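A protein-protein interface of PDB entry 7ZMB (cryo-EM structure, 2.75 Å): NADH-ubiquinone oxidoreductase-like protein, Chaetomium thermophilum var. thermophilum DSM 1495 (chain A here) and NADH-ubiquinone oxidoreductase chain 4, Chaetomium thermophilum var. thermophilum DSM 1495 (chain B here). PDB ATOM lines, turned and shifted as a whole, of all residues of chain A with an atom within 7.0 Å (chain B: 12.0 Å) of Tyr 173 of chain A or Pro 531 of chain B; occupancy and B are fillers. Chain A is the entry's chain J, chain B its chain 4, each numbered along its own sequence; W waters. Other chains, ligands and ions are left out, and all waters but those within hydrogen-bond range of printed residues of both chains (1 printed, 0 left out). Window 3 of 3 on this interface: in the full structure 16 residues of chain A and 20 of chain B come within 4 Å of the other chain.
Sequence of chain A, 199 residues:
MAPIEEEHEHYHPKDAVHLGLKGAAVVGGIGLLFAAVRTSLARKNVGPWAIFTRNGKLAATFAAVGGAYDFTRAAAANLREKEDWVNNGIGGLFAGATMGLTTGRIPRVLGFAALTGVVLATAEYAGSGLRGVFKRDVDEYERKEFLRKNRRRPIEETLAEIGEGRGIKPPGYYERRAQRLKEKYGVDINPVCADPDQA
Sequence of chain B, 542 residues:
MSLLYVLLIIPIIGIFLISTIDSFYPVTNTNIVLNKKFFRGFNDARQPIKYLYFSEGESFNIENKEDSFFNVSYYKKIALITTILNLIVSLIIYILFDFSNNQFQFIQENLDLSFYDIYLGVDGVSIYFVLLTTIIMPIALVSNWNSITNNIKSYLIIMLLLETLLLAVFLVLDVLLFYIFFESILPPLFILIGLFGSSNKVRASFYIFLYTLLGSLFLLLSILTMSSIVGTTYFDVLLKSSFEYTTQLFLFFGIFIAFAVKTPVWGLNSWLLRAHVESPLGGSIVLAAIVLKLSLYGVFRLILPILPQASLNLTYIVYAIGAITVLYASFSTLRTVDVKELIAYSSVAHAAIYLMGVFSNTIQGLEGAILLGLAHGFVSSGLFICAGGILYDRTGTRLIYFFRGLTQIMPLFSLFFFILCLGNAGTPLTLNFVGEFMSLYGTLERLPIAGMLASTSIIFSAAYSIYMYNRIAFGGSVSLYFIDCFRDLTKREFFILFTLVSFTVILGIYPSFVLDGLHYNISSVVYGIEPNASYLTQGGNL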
ATOM      1  N   GLU A 164      28.776  -0.792 -23.997  1.00  0.00           N
ATOM      2  CA  GLU A 164      27.948  -1.971 -24.162  1.00  0.00           C
ATOM      3  C   GLU A 164      27.289  -2.250 -22.823  1.00  0.00           C
ATOM      4  O   GLU A 164      27.914  -2.083 -21.774  1.00  0.00           O
ATOM      5  CB  GLU A 164      28.792  -3.155 -24.641  1.00  0.00           C
ATOM      6  CG  GLU A 164      28.018  -4.300 -25.239  1.00  0.00           C
ATOM      7  CD  GLU A 164      28.901  -5.505 -25.497  1.00  0.00           C
ATOM      8  OE1 GLU A 164      28.369  -6.589 -25.809  1.00  0.00           O
ATOM      9  OE2 GLU A 164      30.137  -5.366 -25.387  1.00  0.00           O
ATOM     10  N   GLY A 165      26.035  -2.654 -22.862  1.00  0.00           N
ATOM     11  CA  GLY A 165      25.251  -2.714 -21.655  1.00  0.00           C
ATOM     12  C   GLY A 165      24.481  -1.434 -21.424  1.00  0.00           C
ATOM     13  O   GLY A 165      24.415  -0.540 -22.271  1.00  0.00           O
ATOM     14  N   ARG A 166      23.892  -1.347 -20.232  1.00  0.00           N
ATOM     15  CA  ARG A 166      22.932  -0.291 -19.904  1.00  0.00           C
ATOM     16  C   ARG A 166      21.817  -0.244 -20.942  1.00  0.00           C
ATOM     17  O   ARG A 166      21.398   0.822 -21.388  1.00  0.00           O
ATOM     18  CB  ARG A 166      23.613   1.073 -19.779  1.00  0.00           C
ATOM     19  CG  ARG A 166      24.960   1.030 -19.125  1.00  0.00           C
ATOM     20  CD  ARG A 166      25.479   2.418 -18.866  1.00  0.00           C
ATOM     21  NE  ARG A 166      25.952   3.073 -20.078  1.00  0.00           N
ATOM     22  CZ  ARG A 166      26.605   4.227 -20.075  1.00  0.00           C
ATOM     23  NH1 ARG A 166      27.019   4.773 -21.208  1.00  0.00           N
ATOM     24  NH2 ARG A 166      26.846   4.831 -18.929  1.00  0.00           N
ATOM     25  N   GLY A 167      21.339  -1.416 -21.332  1.00  0.00           N
ATOM     26  CA  GLY A 167      20.366  -1.539 -22.385  1.00  0.00           C
ATOM     27  C   GLY A 167      20.954  -1.773 -23.756  1.00  0.00           C
ATOM     28  O   GLY A 167      20.226  -2.174 -24.666  1.00  0.00           O
ATOM     29  N   ILE A 168      22.246  -1.521 -23.930  1.00  0.00           N
ATOM     30  CA  ILE A 168      22.930  -1.830 -25.194  1.00  0.00           C
ATOM     31  C   ILE A 168      23.461  -3.248 -25.041  1.00  0.00           C
ATOM     32  O   ILE A 168      24.610  -3.494 -24.674  1.00  0.00           O
ATOM     33  CB  ILE A 168      24.026  -0.816 -25.523  1.00  0.00           C
ATOM     34  CG1 ILE A 168      23.514   0.604 -25.284  1.00  0.00           C
ATOM     35  CG2 ILE A 168      24.489  -0.984 -26.950  1.00  0.00           C
ATOM     36  CD1 ILE A 168      22.284   0.957 -26.077  1.00  0.00           C
ATOM     37  N   LYS A 169      22.590  -4.213 -25.320  1.00  0.00           N
ATOM     38  CA  LYS A 169      22.927  -5.627 -25.197  1.00  0.00           C
ATOM     39  C   LYS A 169      22.858  -6.223 -26.591  1.00  0.00           C
ATOM     40  O   LYS A 169      21.803  -6.707 -27.019  1.00  0.00           O
ATOM     41  CB  LYS A 169      21.975  -6.337 -24.234  1.00  0.00           C
ATOM     42  CG  LYS A 169      21.971  -5.716 -22.851  1.00  0.00           C
ATOM     43  CD  LYS A 169      21.970  -6.767 -21.752  1.00  0.00           C
ATOM     44  CE  LYS A 169      20.730  -7.642 -21.798  1.00  0.00           C
ATOM     45  NZ  LYS A 169      19.497  -6.876 -21.465  1.00  0.00           N
ATOM     46  N   PRO A 170      23.950  -6.185 -27.347  1.00  0.00           N
ATOM     47  CA  PRO A 170      23.911  -6.582 -28.746  1.00  0.00           C
ATOM     48  C   PRO A 170      23.913  -8.093 -28.860  1.00  0.00           C
ATOM     49  O   PRO A 170      24.177  -8.784 -27.867  1.00  0.00           O
ATOM     50  CB  PRO A 170      25.206  -5.973 -29.310  1.00  0.00           C
ATOM     51  CG  PRO A 170      25.669  -5.001 -28.277  1.00  0.00           C
ATOM     52  CD  PRO A 170      25.246  -5.596 -26.994  1.00  0.00           C
ATOM     53  N   PRO A 171      23.645  -8.651 -30.040  1.00  0.00           N
ATOM     54  CA  PRO A 171      23.788 -10.100 -30.180  1.00  0.00           C
ATOM     55  C   PRO A 171      25.223 -10.521 -29.910  1.00  0.00           C
ATOM     56  O   PRO A 171      26.168 -10.012 -30.515  1.00  0.00           O
ATOM     57  CB  PRO A 171      23.355 -10.353 -31.624  1.00  0.00           C
ATOM     58  CG  PRO A 171      23.787  -9.145 -32.337  1.00  0.00           C
ATOM     59  CD  PRO A 171      23.595  -7.997 -31.360  1.00  0.00           C
ATOM     60  N   GLY A 172      25.378 -11.442 -28.967  1.00  0.00           N
ATOM     61  CA  GLY A 172      26.679 -11.784 -28.442  1.00  0.00           C
ATOM     62  C   GLY A 172      27.022 -11.145 -27.116  1.00  0.00           C
ATOM     63  O   GLY A 172      28.155 -11.308 -26.649  1.00  0.00           O
ATOM     64  N   TYR A 173      26.087 -10.414 -26.500  1.00  0.00           N
ATOM     65  CA  TYR A 173      26.332  -9.873 -25.167  1.00  0.00           C
ATOM     66  C   TYR A 173      26.561 -10.983 -24.154  1.00  0.00           C
ATOM     67  O   TYR A 173      27.466 -10.894 -23.320  1.00  0.00           O
ATOM     68  CB  TYR A 173      25.164  -8.997 -24.721  1.00  0.00           C
ATOM     69  CG  TYR A 173      25.490  -8.097 -23.547  1.00  0.00           C
ATOM     70  CD1 TYR A 173      26.327  -7.008 -23.694  1.00  0.00           C
ATOM     71  CD2 TYR A 173      24.979  -8.358 -22.289  1.00  0.00           C
ATOM     72  CE1 TYR A 173      26.632  -6.195 -22.633  1.00  0.00           C
ATOM     73  CE2 TYR A 173      25.281  -7.555 -21.220  1.00  0.00           C
ATOM     74  CZ  TYR A 173      26.107  -6.469 -21.397  1.00  0.00           C
ATOM     75  OH  TYR A 173      26.414  -5.655 -20.332  1.00  0.00           O
ATOM     76  N   TYR A 174      25.752 -12.040 -24.211  1.00  0.00           N
ATOM     77  CA  TYR A 174      25.812 -13.069 -23.182  1.00  0.00           C
ATOM     78  C   TYR A 174      27.019 -13.981 -23.356  1.00  0.00           C
ATOM     79  O   TYR A 174      27.625 -14.404 -22.365  1.00  0.00           O
ATOM     80  CB  TYR A 174      24.516 -13.874 -23.176  1.00  0.00           C
ATOM     81  CG  TYR A 174      23.382 -13.152 -22.486  1.00  0.00           C
ATOM     82  CD1 TYR A 174      23.585 -11.909 -21.901  1.00  0.00           C
ATOM     83  CD2 TYR A 174      22.116 -13.712 -22.410  1.00  0.00           C
ATOM     84  CE1 TYR A 174      22.560 -11.243 -21.266  1.00  0.00           C
ATOM     85  CE2 TYR A 174      21.083 -13.052 -21.776  1.00  0.00           C
ATOM     86  CZ  TYR A 174      21.310 -11.818 -21.206  1.00  0.00           C
ATOM     87  OH  TYR A 174      20.286 -11.154 -20.572  1.00  0.00           O
ATOM     88  N   GLU A 175      27.383 -14.301 -24.599  1.00  0.00           N
ATOM     89  CA  GLU A 175      28.547 -15.150 -24.823  1.00  0.00           C
ATOM     90  C   GLU A 175      29.821 -14.481 -24.325  1.00  0.00           C
ATOM     91  O   GLU A 175      30.662 -15.124 -23.686  1.00  0.00           O
ATOM     92  CB  GLU A 175      28.666 -15.499 -26.306  1.00  0.00           C
ATOM     93  N   ARG A 176      29.979 -13.186 -24.602  1.00  0.00           N
ATOM     94  CA  ARG A 176      31.163 -12.465 -24.151  1.00  0.00           C
ATOM     95  C   ARG A 176      31.096 -12.115 -22.670  1.00  0.00           C
ATOM     96  O   ARG A 176      32.139 -12.044 -22.010  1.00  0.00           O
ATOM     97  CB  ARG A 176      31.357 -11.199 -24.984  1.00  0.00           C
ATOM     98  CG  ARG A 176      32.080 -11.437 -26.298  1.00  0.00           C
ATOM     99  CD  ARG A 176      32.521 -10.125 -26.936  1.00  0.00           C
ATOM    100  NE  ARG A 176      31.430  -9.160 -27.083  1.00  0.00           N
ATOM    101  CZ  ARG A 176      30.327  -9.355 -27.802  1.00  0.00           C
ATOM    102  NH1 ARG A 176      29.403  -8.408 -27.857  1.00  0.00           N
ATOM    103  NH2 ARG A 176      30.151 -10.477 -28.489  1.00  0.00           N
ATOM    104  N   ARG A 177      29.895 -11.888 -22.137  1.00  0.00           N
ATOM    105  CA  ARG A 177      29.766 -11.546 -20.723  1.00  0.00           C
ATOM    106  C   ARG A 177      30.254 -12.684 -19.839  1.00  0.00           C
ATOM    107  O   ARG A 177      30.901 -12.449 -18.813  1.00  0.00           O
ATOM    108  CB  ARG A 177      28.316 -11.198 -20.394  1.00  0.00           C
ATOM    109  CG  ARG A 177      28.084 -10.745 -18.968  1.00  0.00           C
ATOM    110  CD  ARG A 177      26.621 -10.424 -18.735  1.00  0.00           C
ATOM    111  NE  ARG A 177      26.249 -10.576 -17.332  1.00  0.00           N
ATOM    112  CZ  ARG A 177      25.948 -11.738 -16.762  1.00  0.00           C
ATOM    113  NH1 ARG A 177      25.621 -11.784 -15.478  1.00  0.00           N
ATOM    114  NH2 ARG A 177      25.971 -12.855 -17.477  1.00  0.00           N
ATOM    115  N   ALA A 178      29.948 -13.926 -20.220  1.00  0.00           N
ATOM    116  CA  ALA A 178      30.418 -15.069 -19.448  1.00  0.00           C
ATOM    117  C   ALA A 178      31.939 -15.123 -19.421  1.00  0.00           C
ATOM    118  O   ALA A 178      32.540 -15.382 -18.373  1.00  0.00           O
ATOM    119  CB  ALA A 178      29.844 -16.362 -20.023  1.00  0.00           C
ATOM    120  N   ARG A 180      34.006 -12.532 -19.893  1.00  0.00           N
ATOM    121  CA  ARG A 180      34.531 -11.370 -19.182  1.00  0.00           C
ATOM    122  C   ARG A 180      34.464 -11.565 -17.674  1.00  0.00           C
ATOM    123  O   ARG A 180      35.404 -11.214 -16.952  1.00  0.00           O
ATOM    124  CB  ARG A 180      33.769 -10.113 -19.596  1.00  0.00           C
ATOM    125  CG  ARG A 180      34.339  -8.830 -19.017  1.00  0.00           C
ATOM    126  CD  ARG A 180      33.896  -7.616 -19.816  1.00  0.00           C
ATOM    127  NE  ARG A 180      32.512  -7.730 -20.262  1.00  0.00           N
ATOM    128  CZ  ARG A 180      31.468  -7.288 -19.569  1.00  0.00           C
ATOM    129  NH1 ARG A 180      30.242  -7.432 -20.050  1.00  0.00           N
ATOM    130  NH2 ARG A 180      31.650  -6.701 -18.395  1.00  0.00           N
ATOM    131  N   LEU B 312      22.716   8.713 -23.077  1.00  0.00           N
ATOM    132  CA  LEU B 312      23.124   7.490 -22.396  1.00  0.00           C
ATOM    133  C   LEU B 312      24.426   7.673 -21.630  1.00  0.00           C
ATOM    134  O   LEU B 312      24.667   6.967 -20.645  1.00  0.00           O
ATOM    135  CB  LEU B 312      23.261   6.350 -23.404  1.00  0.00           C
ATOM    136  CG  LEU B 312      23.345   4.947 -22.799  1.00  0.00           C
ATOM    137  CD1 LEU B 312      21.988   4.492 -22.317  1.00  0.00           C
ATOM    138  CD2 LEU B 312      23.922   3.966 -23.789  1.00  0.00           C
ATOM    139  N   GLU B 445      16.294   1.410 -11.685  1.00  0.00           N
ATOM    140  CA  GLU B 445      16.714   0.381 -12.630  1.00  0.00           C
ATOM    141  C   GLU B 445      17.809   0.882 -13.563  1.00  0.00           C
ATOM    142  O   GLU B 445      18.612   0.086 -14.058  1.00  0.00           O
ATOM    143  CB  GLU B 445      15.507  -0.110 -13.434  1.00  0.00           C
ATOM    144  CG  GLU B 445      15.801  -1.262 -14.374  1.00  0.00           C
ATOM    145  CD  GLU B 445      14.624  -1.622 -15.262  1.00  0.00           C
ATOM    146  OE1 GLU B 445      13.924  -0.709 -15.719  1.00  0.00           O
ATOM    147  OE2 GLU B 445      14.400  -2.823 -15.506  1.00  0.00           O
ATOM    148  N   ARG B 446      17.866   2.188 -13.813  1.00  0.00           N
ATOM    149  CA  ARG B 446      18.886   2.749 -14.690  1.00  0.00           C
ATOM    150  C   ARG B 446      20.182   3.040 -13.939  1.00  0.00           C
ATOM    151  O   ARG B 446      21.270   2.726 -14.428  1.00  0.00           O
ATOM    152  CB  ARG B 446      18.347   4.014 -15.367  1.00  0.00           C
ATOM    153  CG  ARG B 446      19.401   4.918 -15.958  1.00  0.00           C
ATOM    154  CD  ARG B 446      19.852   4.411 -17.305  1.00  0.00           C
ATOM    155  NE  ARG B 446      21.092   5.030 -17.763  1.00  0.00           N
ATOM    156  CZ  ARG B 446      22.304   4.667 -17.361  1.00  0.00           C
ATOM    157  NH1 ARG B 446      23.371   5.275 -17.842  1.00  0.00           N
ATOM    158  NH2 ARG B 446      22.449   3.689 -16.482  1.00  0.00           N
ATOM    159  N   TYR B 527      16.010   3.572 -26.197  1.00  0.00           N
ATOM    160  CA  TYR B 527      17.256   3.367 -26.975  1.00  0.00           C
ATOM    161  C   TYR B 527      17.938   2.082 -26.516  1.00  0.00           C
ATOM    162  O   TYR B 527      18.435   2.040 -25.387  1.00  0.00           O
ATOM    163  CB  TYR B 527      18.210   4.540 -26.764  1.00  0.00           C
ATOM    164  CG  TYR B 527      19.458   4.501 -27.603  1.00  0.00           C
ATOM    165  CD1 TYR B 527      19.386   4.420 -28.982  1.00  0.00           C
ATOM    166  CD2 TYR B 527      20.709   4.550 -27.012  1.00  0.00           C
ATOM    167  CE1 TYR B 527      20.532   4.389 -29.758  1.00  0.00           C
ATOM    168  CE2 TYR B 527      21.863   4.518 -27.772  1.00  0.00           C
ATOM    169  CZ  TYR B 527      21.772   4.440 -29.148  1.00  0.00           C
ATOM    170  OH  TYR B 527      22.909   4.389 -29.893  1.00  0.00           O
ATOM    171  N   GLY B 528      17.976   1.065 -27.370  1.00  0.00           N
ATOM    172  CA  GLY B 528      18.721  -0.150 -27.003  1.00  0.00           C
ATOM    173  C   GLY B 528      18.161  -1.390 -27.655  1.00  0.00           C
ATOM    174  O   GLY B 528      17.160  -1.269 -28.378  1.00  0.00           O
ATOM    175  N   ILE B 529      18.788  -2.539 -27.405  1.00  0.00           N
ATOM    176  CA  ILE B 529      18.376  -3.796 -28.090  1.00  0.00           C
ATOM    177  C   ILE B 529      18.700  -4.972 -27.174  1.00  0.00           C
ATOM    178  O   ILE B 529      19.562  -4.813 -26.301  1.00  0.00           O
ATOM    179  CB  ILE B 529      19.108  -3.948 -29.439  1.00  0.00           C
ATOM    180  CG1 ILE B 529      20.622  -3.787 -29.283  1.00  0.00           C
ATOM    181  CG2 ILE B 529      18.540  -3.006 -30.488  1.00  0.00           C
ATOM    182  CD1 ILE B 529      21.412  -4.312 -30.457  1.00  0.00           C
ATOM    183  N   GLU B 530      18.026  -6.101 -27.375  1.00  0.00           N
ATOM    184  CA  GLU B 530      18.345  -7.318 -26.597  1.00  0.00           C
ATOM    185  C   GLU B 530      19.104  -8.298 -27.514  1.00  0.00           C
ATOM    186  O   GLU B 530      18.765  -8.343 -28.711  1.00  0.00           O
ATOM    187  CB  GLU B 530      17.059  -7.954 -26.066  1.00  0.00           C
ATOM    188  CG  GLU B 530      16.279  -7.047 -25.133  1.00  0.00           C
ATOM    189  CD  GLU B 530      16.934  -6.836 -23.780  1.00  0.00           C
ATOM    190  OE1 GLU B 530      17.370  -7.835 -23.176  1.00  0.00           O
ATOM    191  OE2 GLU B 530      17.017  -5.673 -23.338  1.00  0.00           O
ATOM    192  N   PRO B 531      20.099  -9.086 -27.031  1.00  0.00           N
ATOM    193  CA  PRO B 531      20.887  -9.972 -27.905  1.00  0.00           C
ATOM    194  C   PRO B 531      20.058 -10.974 -28.684  1.00  0.00           C
ATOM    195  O   PRO B 531      20.459 -11.363 -29.787  1.00  0.00           O
ATOM    196  CB  PRO B 531      21.836 -10.671 -26.924  1.00  0.00           C
ATOM    197  CG  PRO B 531      21.850  -9.798 -25.716  1.00  0.00           C
ATOM    198  CD  PRO B 531      20.478  -9.236 -25.620  1.00  0.00           C
ATOM    199  N   ASN B 532      18.919 -11.413 -28.151  1.00  0.00           N
ATOM    200  CA  ASN B 532      18.120 -12.453 -28.787  1.00  0.00           C
ATOM    201  C   ASN B 532      16.846 -11.920 -29.428  1.00  0.00           C
ATOM    202  O   ASN B 532      16.018 -12.714 -29.886  1.00  0.00           O
ATOM    203  CB  ASN B 532      17.778 -13.546 -27.774  1.00  0.00           C
ATOM    204  CG  ASN B 532      19.001 -14.299 -27.296  1.00  0.00           C
ATOM    205  OD1 ASN B 532      19.829 -14.731 -28.098  1.00  0.00           O
ATOM    206  ND2 ASN B 532      19.119 -14.466 -25.985  1.00  0.00           N
ATOM    207  N   ALA B 533      16.664 -10.599 -29.479  1.00  0.00           N
ATOM    208  CA  ALA B 533      15.469 -10.041 -30.100  1.00  0.00           C
ATOM    209  C   ALA B 533      15.798  -8.940 -31.103  1.00  0.00           C
ATOM    210  O   ALA B 533      14.880  -8.310 -31.641  1.00  0.00           O
ATOM    211  CB  ALA B 533      14.505  -9.498 -29.040  1.00  0.00           C
ATOM    212  N   SER B 534      17.075  -8.696 -31.375  1.00  0.00           N
ATOM    213  CA  SER B 534      17.497  -7.674 -32.320  1.00  0.00           C
ATOM    214  C   SER B 534      17.828  -8.319 -33.654  1.00  0.00           C
ATOM    215  O   SER B 534      18.332  -9.445 -33.700  1.00  0.00           O
ATOM    216  CB  SER B 534      18.714  -6.910 -31.801  1.00  0.00           C
ATOM    217  OG  SER B 534      19.778  -7.793 -31.497  1.00  0.00           O
ATOM    218  N   TYR B 535      17.532  -7.601 -34.735  1.00  0.00           N
ATOM    219  CA  TYR B 535      17.874  -8.032 -36.090  1.00  0.00           C
ATOM    220  C   TYR B 535      17.271  -9.397 -36.421  1.00  0.00           C
ATOM    221  O   TYR B 535      17.953 -10.301 -36.909  1.00  0.00           O
ATOM    222  CB  TYR B 535      19.390  -8.047 -36.286  1.00  0.00           C
ATOM    223  CG  TYR B 535      20.072  -6.796 -35.812  1.00  0.00           C
ATOM    224  CD1 TYR B 535      19.941  -5.609 -36.509  1.00  0.00           C
ATOM    225  CD2 TYR B 535      20.849  -6.802 -34.676  1.00  0.00           C
ATOM    226  CE1 TYR B 535      20.562  -4.461 -36.080  1.00  0.00           C
ATOM    227  CE2 TYR B 535      21.473  -5.660 -34.241  1.00  0.00           C
ATOM    228  CZ  TYR B 535      21.326  -4.494 -34.945  1.00  0.00           C
ATOM    229  OH  TYR B 535      21.955  -3.352 -34.519  1.00  0.00           O
ATOM    230  N   LEU B 536      15.978  -9.545 -36.147  1.00  0.00           N
ATOM    231  CA  LEU B 536      15.274 -10.758 -36.536  1.00  0.00           C
ATOM    232  C   LEU B 536      15.185 -10.850 -38.054  1.00  0.00           C
ATOM    233  O   LEU B 536      14.906  -9.862 -38.737  1.00  0.00           O
ATOM    234  CB  LEU B 536      13.875 -10.782 -35.925  1.00  0.00           C
ATOM    235  CG  LEU B 536      13.802 -10.733 -34.398  1.00  0.00           C
ATOM    236  CD1 LEU B 536      12.356 -10.742 -33.929  1.00  0.00           C
ATOM    237  CD2 LEU B 536      14.568 -11.895 -33.793  1.00  0.00           C
ATOM    238  N   THR B 537      15.427 -12.045 -38.582  1.00  0.00           N
ATOM    239  CA  THR B 537      15.372 -12.266 -40.023  1.00  0.00           C
ATOM    240  C   THR B 537      14.464 -13.444 -40.361  1.00  0.00           C
ATOM    241  O   THR B 537      13.848 -13.478 -41.427  1.00  0.00           O
ATOM    242  CB  THR B 537      16.772 -12.520 -40.612  1.00  0.00           C
ATOM    243  OG1 THR B 537      17.393 -13.613 -39.924  1.00  0.00           O
ATOM    244  CG2 THR B 537      17.641 -11.282 -40.477  1.00  0.00           C
HETATM  245  O   HOH W   1      25.760   7.822 -17.591  1.00  0.00           O
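Arg 446 of chain B touches Arg 166 of chain A. O of Gly 167 of chain A touches CA of Gly 528 of chain B, 3.4 Å away. Leu 312 of chain B touches Ile 168 of chain A (CD2 to CG1, 3.7 Å). Ile 168 of chain A touches Tyr 527 of chain B. CD1 of Ile 168 of chain A touches CA of Gly 528 of chain B (3.8 Å). Pro 170 of chain A touches Ile 529 of chain B (CA to CD1, 3.8 Å). Pro 170 of chain A touches Pro 531 of chain B. Pro 531 of chain B touches Pro 171 of chain A. CD of Pro 171 of chain A touches OG of Ser 534 of chain B, 3.8 Å away. Tyr 173 of chain A touches Pro 531 of chain B.
The backbone carbonyl oxygen (O) of Glu 530 of chain B is in hydrogen-bond range of the side-chain hydroxyl (OG) of Ser 534 of chain B (3.0 Å).
The side-chain carboxylate (OE1) of Glu 530 of chain B is in salt-bridge range of the side-chain amino group (NZ) of Lys 169 of chain A (2.9 Å). The backbone carbonyl oxygen (O) of Lys 169 of chain A sits close to the backbone nitrogen (N) of Pro 531 of chain B, 2.9 Å away. The backbone carbonyl oxygen (O) of Gly 167 of chain A is in hydrogen-bond range of the backbone NH (N) of Ile 529 of chain B (3.1 Å). The backbone NH (N) of Lys 169 of chain A lies within hydrogen-bond range of the backbone carbonyl oxygen (O) of Ile 529 of chain B (3.2 Å). The backbone carbonyl oxygen (O) of Leu 312 of chain B sits at hydrogen-bond distance from the guanidinium group (NH1) of Arg 166 of chain A (3.3 Å).
Hydrophobic or aromatic side chains of chain B that line the printed part of chain A: Leu 312, Tyr 527, Ile 529 and Pro 531. Along chain B the printed residues that touch a printed residue of chain A span positions 312 to 534.
Water W1 lies within hydrogen-bond range of the backbone carbonyl oxygen (O) of Leu 312 of chain B (3.4 Å) and the guanidinium group (NH2) of Arg 166 of chain A (3.5 Å).
Glu 164 of chain A touches none of the printed residues of chain B. Gly 165 of chain A touches none of the printed residues of chain B. Of the printed residues of chain B, Arg 166 of chain A touches Leu 312 (3.3 Å) and Arg 446 (3.7 Å). Gly 167 of chain A touches just these residues of chain B: Gly 528 and Ile 529. Of chain B, only Ile 529 and Pro 531 come within 4 Å of Pro 170 of chain A. No residue of chain B comes within 4 Å of Gly 172 of chain A. Of chain B, only Pro 531 comes within 4 Å of Tyr 173 of chain A. No residue of chain B comes within 4 Å of Tyr 174 of chain A. No residue of chain B comes within 4 Å of Glu 175 of chain A. No residue of chain B comes within 4 Å of Arg 177 of chain A. Ala 178 of chain A touches none of the printed residues of chain B. Of the printed residues of chain A, Glu 530 of chain B touches Lys 169. Of chain A, only Lys 169 (2.9 Å), Pro 170 (3.2 Å), Pro 171 (3.6 Å) and Tyr 173 (3.6 Å) come within 4 Å of Pro 531 of chain B. Ala 533 of chain B touches none of the printed residues of chain A. The nearest residue of chain B that does not touch Tyr 173 of chain A is Glu 530 of chain B (6.7 Å). The nearest residue of chain A that does not touch Pro 531 of chain B is Gly 172 of chain A (4.2 Å).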
